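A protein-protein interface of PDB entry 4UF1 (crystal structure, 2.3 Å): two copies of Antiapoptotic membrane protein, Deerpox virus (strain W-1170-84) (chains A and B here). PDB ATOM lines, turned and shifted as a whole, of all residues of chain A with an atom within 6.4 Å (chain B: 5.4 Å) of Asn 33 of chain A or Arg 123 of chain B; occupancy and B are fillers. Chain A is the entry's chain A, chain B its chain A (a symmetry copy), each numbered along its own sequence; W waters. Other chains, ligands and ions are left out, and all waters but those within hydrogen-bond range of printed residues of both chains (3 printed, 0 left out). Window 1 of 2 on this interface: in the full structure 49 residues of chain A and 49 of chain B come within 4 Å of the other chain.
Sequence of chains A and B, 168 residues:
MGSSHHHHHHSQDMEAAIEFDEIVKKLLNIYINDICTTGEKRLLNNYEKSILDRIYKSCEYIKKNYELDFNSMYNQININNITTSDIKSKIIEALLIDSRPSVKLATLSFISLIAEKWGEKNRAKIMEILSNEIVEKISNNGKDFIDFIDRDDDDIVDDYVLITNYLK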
ATOM      1  N   LEU A  28      21.137  12.620  33.017  1.00  0.00           N
ATOM      2  CA  LEU A  28      22.347  12.094  32.389  1.00  0.00           C
ATOM      3  C   LEU A  28      22.786  12.971  31.219  1.00  0.00           C
ATOM      4  O   LEU A  28      23.979  13.153  30.998  1.00  0.00           O
ATOM      5  CB  LEU A  28      22.138  10.652  31.915  1.00  0.00           C
ATOM      6  CG  LEU A  28      22.077   9.549  32.982  1.00  0.00           C
ATOM      7  CD1 LEU A  28      22.130   8.187  32.315  1.00  0.00           C
ATOM      8  CD2 LEU A  28      23.177   9.676  34.026  1.00  0.00           C
ATOM      9  N   ASN A  29      21.829  13.517  30.474  1.00  0.00           N
ATOM     10  CA  ASN A  29      22.154  14.436  29.387  1.00  0.00           C
ATOM     11  C   ASN A  29      22.749  15.736  29.921  1.00  0.00           C
ATOM     12  O   ASN A  29      23.746  16.222  29.393  1.00  0.00           O
ATOM     13  CB  ASN A  29      20.920  14.737  28.535  1.00  0.00           C
ATOM     14  CG  ASN A  29      20.656  13.671  27.489  1.00  0.00           C
ATOM     15  OD1 ASN A  29      21.315  13.629  26.452  1.00  0.00           O
ATOM     16  ND2 ASN A  29      19.678  12.813  27.751  1.00  0.00           N
ATOM     17  N   ILE A  30      22.142  16.299  30.964  1.00  0.00           N
ATOM     18  CA  ILE A  30      22.678  17.508  31.587  1.00  0.00           C
ATOM     19  C   ILE A  30      24.073  17.239  32.134  1.00  0.00           C
ATOM     20  O   ILE A  30      24.976  18.065  31.991  1.00  0.00           O
ATOM     21  CB  ILE A  30      21.785  18.028  32.736  1.00  0.00           C
ATOM     22  CG1 ILE A  30      20.464  18.569  32.188  1.00  0.00           C
ATOM     23  CG2 ILE A  30      22.494  19.148  33.507  1.00  0.00           C
ATOM     24  CD1 ILE A  30      19.407  18.809  33.258  1.00  0.00           C
ATOM     25  N   TYR A  31      24.244  16.081  32.765  1.00  0.00           N
ATOM     26  CA  TYR A  31      25.498  15.761  33.426  1.00  0.00           C
ATOM     27  C   TYR A  31      26.651  15.656  32.424  1.00  0.00           C
ATOM     28  O   TYR A  31      27.702  16.260  32.620  1.00  0.00           O
ATOM     29  CB  TYR A  31      25.374  14.457  34.219  1.00  0.00           C
ATOM     30  CG  TYR A  31      26.712  13.904  34.657  1.00  0.00           C
ATOM     31  CD1 TYR A  31      27.500  14.588  35.574  1.00  0.00           C
ATOM     32  CD2 TYR A  31      27.194  12.708  34.143  1.00  0.00           C
ATOM     33  CE1 TYR A  31      28.728  14.095  35.968  1.00  0.00           C
ATOM     34  CE2 TYR A  31      28.425  12.206  34.534  1.00  0.00           C
ATOM     35  CZ  TYR A  31      29.184  12.903  35.445  1.00  0.00           C
ATOM     36  OH  TYR A  31      30.406  12.406  35.835  1.00  0.00           O
ATOM     37  N   ILE A  32      26.451  14.906  31.345  1.00  0.00           N
ATOM     38  CA  ILE A  32      27.529  14.655  30.397  1.00  0.00           C
ATOM     39  C   ILE A  32      27.795  15.879  29.516  1.00  0.00           C
ATOM     40  O   ILE A  32      28.928  16.094  29.091  1.00  0.00           O
ATOM     41  CB  ILE A  32      27.218  13.416  29.526  1.00  0.00           C
ATOM     42  CG1 ILE A  32      27.211  12.150  30.391  1.00  0.00           C
ATOM     43  CG2 ILE A  32      28.232  13.261  28.386  1.00  0.00           C
ATOM     44  CD1 ILE A  32      28.547  11.832  31.063  1.00  0.00           C
ATOM     45  N   ASN A  33      26.773  16.687  29.247  1.00  0.00           N
ATOM     46  CA  ASN A  33      26.997  17.947  28.540  1.00  0.00           C
ATOM     47  C   ASN A  33      27.893  18.881  29.354  1.00  0.00           C
ATOM     48  O   ASN A  33      28.711  19.611  28.797  1.00  0.00           O
ATOM     49  CB  ASN A  33      25.680  18.656  28.218  1.00  0.00           C
ATOM     50  CG  ASN A  33      25.173  18.348  26.817  1.00  0.00           C
ATOM     51  OD1 ASN A  33      25.754  18.789  25.822  1.00  0.00           O
ATOM     52  ND2 ASN A  33      24.077  17.602  26.735  1.00  0.00           N
ATOM     53  N   ASP A  34      27.737  18.852  30.674  1.00  0.00           N
ATOM     54  CA  ASP A  34      28.544  19.697  31.549  1.00  0.00           C
ATOM     55  C   ASP A  34      29.992  19.210  31.608  1.00  0.00           C
ATOM     56  O   ASP A  34      30.917  20.019  31.604  1.00  0.00           O
ATOM     57  CB  ASP A  34      27.950  19.741  32.956  1.00  0.00           C
ATOM     58  CG  ASP A  34      28.456  20.917  33.765  1.00  0.00           C
ATOM     59  OD1 ASP A  34      28.565  22.028  33.205  1.00  0.00           O
ATOM     60  OD2 ASP A  34      28.748  20.730  34.964  1.00  0.00           O
ATOM     61  N   ILE A  35      30.192  17.894  31.657  1.00  0.00           N
ATOM     62  CA  ILE A  35      31.546  17.341  31.681  1.00  0.00           C
ATOM     63  C   ILE A  35      32.255  17.686  30.374  1.00  0.00           C
ATOM     64  O   ILE A  35      33.451  17.968  30.367  1.00  0.00           O
ATOM     65  CB  ILE A  35      31.555  15.805  31.887  1.00  0.00           C
ATOM     66  CG1 ILE A  35      30.883  15.419  33.213  1.00  0.00           C
ATOM     67  CG2 ILE A  35      32.981  15.264  31.853  1.00  0.00           C
ATOM     68  CD1 ILE A  35      31.598  15.904  34.467  1.00  0.00           C
ATOM     69  N   CYS A  36      31.509  17.658  29.272  1.00  0.00           N
ATOM     70  CA  CYS A  36      32.028  18.072  27.973  1.00  0.00           C
ATOM     71  C   CYS A  36      32.594  19.489  28.023  1.00  0.00           C
ATOM     72  O   CYS A  36      33.709  19.737  27.560  1.00  0.00           O
ATOM     73  CB  CYS A  36      30.933  17.991  26.907  1.00  0.00           C
ATOM     74  SG  CYS A  36      30.652  16.332  26.258  1.00  0.00           S
ATOM     75  N   THR A  37      31.819  20.409  28.590  1.00  0.00           N
ATOM     76  CA  THR A  37      32.243  21.798  28.735  1.00  0.00           C
ATOM     77  C   THR A  37      33.541  21.880  29.529  1.00  0.00           C
ATOM     78  O   THR A  37      34.466  22.607  29.161  1.00  0.00           O
ATOM     79  CB  THR A  37      31.165  22.649  29.444  1.00  0.00           C
ATOM     80  OG1 THR A  37      29.940  22.598  28.701  1.00  0.00           O
ATOM     81  CG2 THR A  37      31.618  24.104  29.581  1.00  0.00           C
ATOM     82  N   THR A  38      33.592  21.129  30.624  1.00  0.00           N
ATOM     83  CA  THR A  38      34.765  21.096  31.487  1.00  0.00           C
ATOM     84  C   THR A  38      35.972  20.570  30.717  1.00  0.00           C
ATOM     85  O   THR A  38      37.064  21.135  30.794  1.00  0.00           O
ATOM     86  CB  THR A  38      34.512  20.223  32.730  1.00  0.00           C
ATOM     87  OG1 THR A  38      33.450  20.795  33.503  1.00  0.00           O
ATOM     88  CG2 THR A  38      35.761  20.122  33.595  1.00  0.00           C
ATOM     89  N   GLU A  40      36.388  20.785  27.628  1.00  0.00           N
ATOM     90  CA  GLU A  40      36.724  21.808  26.645  1.00  0.00           C
ATOM     91  C   GLU A  40      37.485  22.969  27.287  1.00  0.00           C
ATOM     92  O   GLU A  40      38.491  23.432  26.752  1.00  0.00           O
ATOM     93  CB  GLU A  40      35.453  22.317  25.959  1.00  0.00           C
ATOM     94  CG  GLU A  40      34.883  21.350  24.929  1.00  0.00           C
ATOM     95  CD  GLU A  40      33.408  21.587  24.646  1.00  0.00           C
ATOM     96  OE1 GLU A  40      32.862  22.615  25.105  1.00  0.00           O
ATOM     97  OE2 GLU A  40      32.792  20.738  23.963  1.00  0.00           O
ATOM     98  N   ARG A 123      18.586  21.338  23.963  1.00  0.00           N
ATOM     99  CA  ARG A 123      19.763  22.177  23.761  1.00  0.00           C
ATOM    100  C   ARG A 123      20.012  22.514  22.292  1.00  0.00           C
ATOM    101  O   ARG A 123      20.498  23.598  21.969  1.00  0.00           O
ATOM    102  CB  ARG A 123      20.968  21.455  24.368  1.00  0.00           C
ATOM    103  CG  ARG A 123      22.342  21.895  23.913  1.00  0.00           C
ATOM    104  CD  ARG A 123      23.367  20.958  24.532  1.00  0.00           C
ATOM    105  NE  ARG A 123      23.246  20.928  25.989  1.00  0.00           N
ATOM    106  CZ  ARG A 123      23.954  21.679  26.826  1.00  0.00           C
ATOM    107  NH1 ARG A 123      24.865  22.530  26.371  1.00  0.00           N
ATOM    108  NH2 ARG A 123      23.753  21.570  28.131  1.00  0.00           N
ATOM    109  N   ILE B  30      31.579  27.256  23.463  1.00  0.00           N
ATOM    110  CA  ILE B  30      31.734  26.828  24.851  1.00  0.00           C
ATOM    111  C   ILE B  30      30.839  27.662  25.758  1.00  0.00           C
ATOM    112  O   ILE B  30      30.201  27.135  26.671  1.00  0.00           O
ATOM    113  CB  ILE B  30      33.194  26.947  25.347  1.00  0.00           C
ATOM    114  CG1 ILE B  30      34.085  25.922  24.646  1.00  0.00           C
ATOM    115  CG2 ILE B  30      33.271  26.714  26.861  1.00  0.00           C
ATOM    116  CD1 ILE B  30      35.575  26.170  24.836  1.00  0.00           C
ATOM    117  N   ASN B  33      26.962  26.885  25.221  1.00  0.00           N
ATOM    118  CA  ASN B  33      26.662  25.539  25.708  1.00  0.00           C
ATOM    119  C   ASN B  33      26.571  25.513  27.233  1.00  0.00           C
ATOM    120  O   ASN B  33      25.757  24.788  27.803  1.00  0.00           O
ATOM    121  CB  ASN B  33      27.708  24.524  25.242  1.00  0.00           C
ATOM    122  CG  ASN B  33      27.296  23.795  23.972  1.00  0.00           C
ATOM    123  OD1 ASN B  33      26.377  22.971  23.983  1.00  0.00           O
ATOM    124  ND2 ASN B  33      27.986  24.082  22.873  1.00  0.00           N
ATOM    125  N   THR B  37      23.285  24.707  29.857  1.00  0.00           N
ATOM    126  CA  THR B  37      23.311  23.827  31.020  1.00  0.00           C
ATOM    127  C   THR B  37      22.703  24.523  32.232  1.00  0.00           C
ATOM    128  O   THR B  37      21.904  23.939  32.966  1.00  0.00           O
ATOM    129  CB  THR B  37      24.752  23.384  31.365  1.00  0.00           C
ATOM    130  OG1 THR B  37      25.334  22.710  30.242  1.00  0.00           O
ATOM    131  CG2 THR B  37      24.764  22.455  32.579  1.00  0.00           C
ATOM    132  N   LYS B 121      37.637  17.742  20.552  1.00  0.00           N
ATOM    133  CA  LYS B 121      36.669  17.224  19.591  1.00  0.00           C
ATOM    134  C   LYS B 121      35.366  17.996  19.669  1.00  0.00           C
ATOM    135  O   LYS B 121      35.100  18.686  20.654  1.00  0.00           O
ATOM    136  CB  LYS B 121      36.389  15.741  19.838  1.00  0.00           C
ATOM    137  CG  LYS B 121      37.489  14.805  19.390  1.00  0.00           C
ATOM    138  CD  LYS B 121      37.057  13.365  19.551  1.00  0.00           C
ATOM    139  CE  LYS B 121      38.194  12.391  19.276  1.00  0.00           C
ATOM    140  NZ  LYS B 121      38.385  12.143  17.819  1.00  0.00           N
ATOM    141  N   ASN B 122      34.551  17.871  18.628  1.00  0.00           N
ATOM    142  CA  ASN B 122      33.196  18.394  18.683  1.00  0.00           C
ATOM    143  C   ASN B 122      32.398  17.622  19.721  1.00  0.00           C
ATOM    144  O   ASN B 122      32.395  16.388  19.740  1.00  0.00           O
ATOM    145  CB  ASN B 122      32.512  18.314  17.316  1.00  0.00           C
ATOM    146  CG  ASN B 122      31.072  18.822  17.349  1.00  0.00           C
ATOM    147  OD1 ASN B 122      30.626  19.407  18.339  1.00  0.00           O
ATOM    148  ND2 ASN B 122      30.346  18.609  16.259  1.00  0.00           N
ATOM    149  N   ARG B 123      31.736  18.382  20.586  1.00  0.00           N
ATOM    150  CA  ARG B 123      30.846  17.867  21.622  1.00  0.00           C
ATOM    151  C   ARG B 123      29.918  16.763  21.117  1.00  0.00           C
ATOM    152  O   ARG B 123      29.575  15.841  21.858  1.00  0.00           O
ATOM    153  CB  ARG B 123      30.042  19.042  22.183  1.00  0.00           C
ATOM    154  CG  ARG B 123      28.771  18.718  22.935  1.00  0.00           C
ATOM    155  CD  ARG B 123      28.075  20.026  23.274  1.00  0.00           C
ATOM    156  NE  ARG B 123      28.958  20.915  24.028  1.00  0.00           N
ATOM    157  CZ  ARG B 123      28.994  21.004  25.354  1.00  0.00           C
ATOM    158  NH1 ARG B 123      28.185  20.268  26.107  1.00  0.00           N
ATOM    159  NH2 ARG B 123      29.842  21.843  25.930  1.00  0.00           N
ATOM    160  N   ALA B 124      29.524  16.859  19.851  1.00  0.00           N
ATOM    161  CA  ALA B 124      28.621  15.886  19.247  1.00  0.00           C
ATOM    162  C   ALA B 124      29.187  14.466  19.273  1.00  0.00           C
ATOM    163  O   ALA B 124      28.433  13.501  19.407  1.00  0.00           O
ATOM    164  CB  ALA B 124      28.300  16.291  17.817  1.00  0.00           C
ATOM    165  N   LYS B 125      30.506  14.333  19.152  1.00  0.00           N
ATOM    166  CA  LYS B 125      31.120  13.011  19.068  1.00  0.00           C
ATOM    167  C   LYS B 125      31.256  12.333  20.427  1.00  0.00           C
ATOM    168  O   LYS B 125      31.629  11.161  20.497  1.00  0.00           O
ATOM    169  CB  LYS B 125      32.502  13.083  18.391  1.00  0.00           C
ATOM    170  CG  LYS B 125      32.507  13.152  16.845  1.00  0.00           C
ATOM    171  CD  LYS B 125      31.302  12.477  16.201  1.00  0.00           C
ATOM    172  CE  LYS B 125      31.606  11.869  14.844  1.00  0.00           C
ATOM    173  NZ  LYS B 125      32.308  12.794  13.918  1.00  0.00           N
ATOM    174  N   ILE B 126      30.961  13.059  21.503  1.00  0.00           N
ATOM    175  CA  ILE B 126      30.794  12.429  22.806  1.00  0.00           C
ATOM    176  C   ILE B 126      29.310  12.164  23.033  1.00  0.00           C
ATOM    177  O   ILE B 126      28.925  11.097  23.513  1.00  0.00           O
ATOM    178  CB  ILE B 126      31.333  13.290  23.968  1.00  0.00           C
ATOM    179  CG1 ILE B 126      32.811  13.628  23.767  1.00  0.00           C
ATOM    180  CG2 ILE B 126      31.167  12.552  25.291  1.00  0.00           C
ATOM    181  CD1 ILE B 126      33.064  14.867  22.930  1.00  0.00           C
ATOM    182  N   MET B 127      28.481  13.140  22.682  1.00  0.00           N
ATOM    183  CA  MET B 127      27.054  13.059  22.969  1.00  0.00           C
ATOM    184  C   MET B 127      26.345  11.972  22.159  1.00  0.00           C
ATOM    185  O   MET B 127      25.345  11.424  22.621  1.00  0.00           O
ATOM    186  CB  MET B 127      26.376  14.412  22.716  1.00  0.00           C
ATOM    187  CG  MET B 127      26.751  15.509  23.711  1.00  0.00           C
ATOM    188  SD  MET B 127      26.701  15.011  25.445  1.00  0.00           S
ATOM    189  CE  MET B 127      24.982  14.546  25.641  1.00  0.00           C
ATOM    190  N   GLU B 128      26.842  11.655  20.964  1.00  0.00           N
ATOM    191  CA  GLU B 128      26.196  10.621  20.154  1.00  0.00           C
ATOM    192  C   GLU B 128      26.711   9.223  20.524  1.00  0.00           C
ATOM    193  O   GLU B 128      26.247   8.224  19.973  1.00  0.00           O
ATOM    194  CB  GLU B 128      26.374  10.891  18.652  1.00  0.00           C
ATOM    195  CG  GLU B 128      27.740  10.598  18.052  1.00  0.00           C
ATOM    196  CD  GLU B 128      27.732  10.745  16.537  1.00  0.00           C
ATOM    197  OE1 GLU B 128      26.843  10.156  15.885  1.00  0.00           O
ATOM    198  OE2 GLU B 128      28.602  11.456  15.996  1.00  0.00           O
HETATM  199  O   HOH W   1      31.052  23.372  22.551  1.00  0.00           O
HETATM  200  O   HOH W   2      34.168  18.435  23.560  1.00  0.00           O
HETATM  201  O   HOH W   3      28.003  23.067  30.535  1.00  0.00           O
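Printed residues of chain B that touch a printed residue of chain A: Ile 30, Asn 33, Thr 37, Arg 123, Ile 126 and Met 127. Hydrophobic or aromatic side chains of chain A that line the printed part of chain B: Ile 32. Among the printed residues, 12 pairs touch across the chains. Among the printed residues, Asp or Glu carboxylates within 4 Å of a Lys or Arg side-chain nitrogen of the other chain: Glu 40 of chain A with Arg 123 of chain B (3.2 Å).
The backbone carbonyl oxygen of Asn 33 of chain A lies within hydrogen-bond range of the side-chain hydroxyl of Thr 37 of chain A, at 3.2 Å. The backbone carbonyl oxygen of Asn 33 of chain B is in hydrogen-bond range of the side-chain hydroxyl of Thr 37 of chain B, 3.2 Å away. OD1 of Asn 33 of chain B is in hydrogen-bond range of NE of Arg 123 of chain B (3.3 Å). O of Asn 29 of chain A is in hydrogen-bond range of ND2 of Asn 33 of chain A, at 3.0 Å. The side-chain amide oxygen of Asn 33 of chain A lies within hydrogen-bond range of the guanidinium group of Arg 123 of chain A, at 3.3 Å. The backbone carbonyl oxygen (O) of Ile 32 of chain A is in hydrogen-bond range of the side-chain sulfur (SG) of Cys 36 of chain A (3.3 Å).
NH2 of Arg 123 of chain B sits at hydrogen-bond distance from OG1 of Thr 37 of chain A, 2.9 Å away. NH2 of Arg 123 of chain B is in salt-bridge range of OE1 of Glu 40 of chain A. The guanidinium group (NH1) of Arg 123 of chain A lies within hydrogen-bond range of the backbone carbonyl oxygen (O) of Asn 33 of chain B (2.8 Å). O of Asn 33 of chain A lies within hydrogen-bond range of NH1 of Arg 123 of chain B, 2.8 Å away. NH2 of Arg 123 of chain A lies within hydrogen-bond range of OG1 of Thr 37 of chain B.
Asn 33 of chain A touches Arg 123 of chain B, and with the chains exchanged Arg 123 of chain A touches Asn 33 of chain B. Thr 37 of chain A touches Arg 123 of chain B, and with the chains exchanged Arg 123 of chain A touches Thr 37 of chain B. Of the 12 pairs that touch across the chains among the printed residues, 4 have their exchanged pair printed and touching as well.
Among the printed residues, pairs that only touch across the chains: Asn 29 of chain A with Met 127 of chain B (3.9 Å), Ile 32 of chain A with Met 127 of chain B (3.7 Å), Asn 33 of chain A with Met 127 of chain B (3.4 Å), Asp 34 of chain A with Thr 37 of chain B (3.9 Å), Cys 36 of chain A with Arg 123 of chain B (3.7 Å), Cys 36 of chain A with Ile 126 of chain B (3.9 Å) and Glu 40 of chain A with Ile 30 of chain B (3.6 Å).
Asn 33 of chain A touches two residues of chain B. Arg 123 of chain B touches four residues of chain A. Of the printed residues of chain A, Thr 37 of chain B touches Asp 34 and Arg 123. Of the printed residues of chain A, Asn 33 of chain B touches Arg 123 (2.8 Å). Of the printed residues of chain B, Cys 36 of chain A touches Arg 123 and Ile 126. Thr 38 of chain A touches none of the printed residues of chain B. The nearest residue of chain B that does not touch Asn 33 of chain A is Thr 37 of chain B (4.5 Å). The nearest residue of chain A that does not touch Arg 123 of chain B is Arg 123 of chain A (4.03 Å).
Water W3 lies within hydrogen-bond range of the side-chain hydroxyl (OG1) of Thr 37 of chain A (2.7 Å), the side-chain hydroxyl (OG1) of Thr 37 of chain B (2.7 Å) and the side-chain carboxylate (OD1) of Asp 34 of chain A (2.9 Å). Water W2 bridges the side-chain carboxylate of Glu 40 of chain A (2.7 Å) and the backbone carbonyl oxygen of Lys 121 of chain B (3.1 Å). Water W1 lies within hydrogen-bond range of ND2 of Asn 33 of chain B and OE1 of Glu 40 of chain A.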
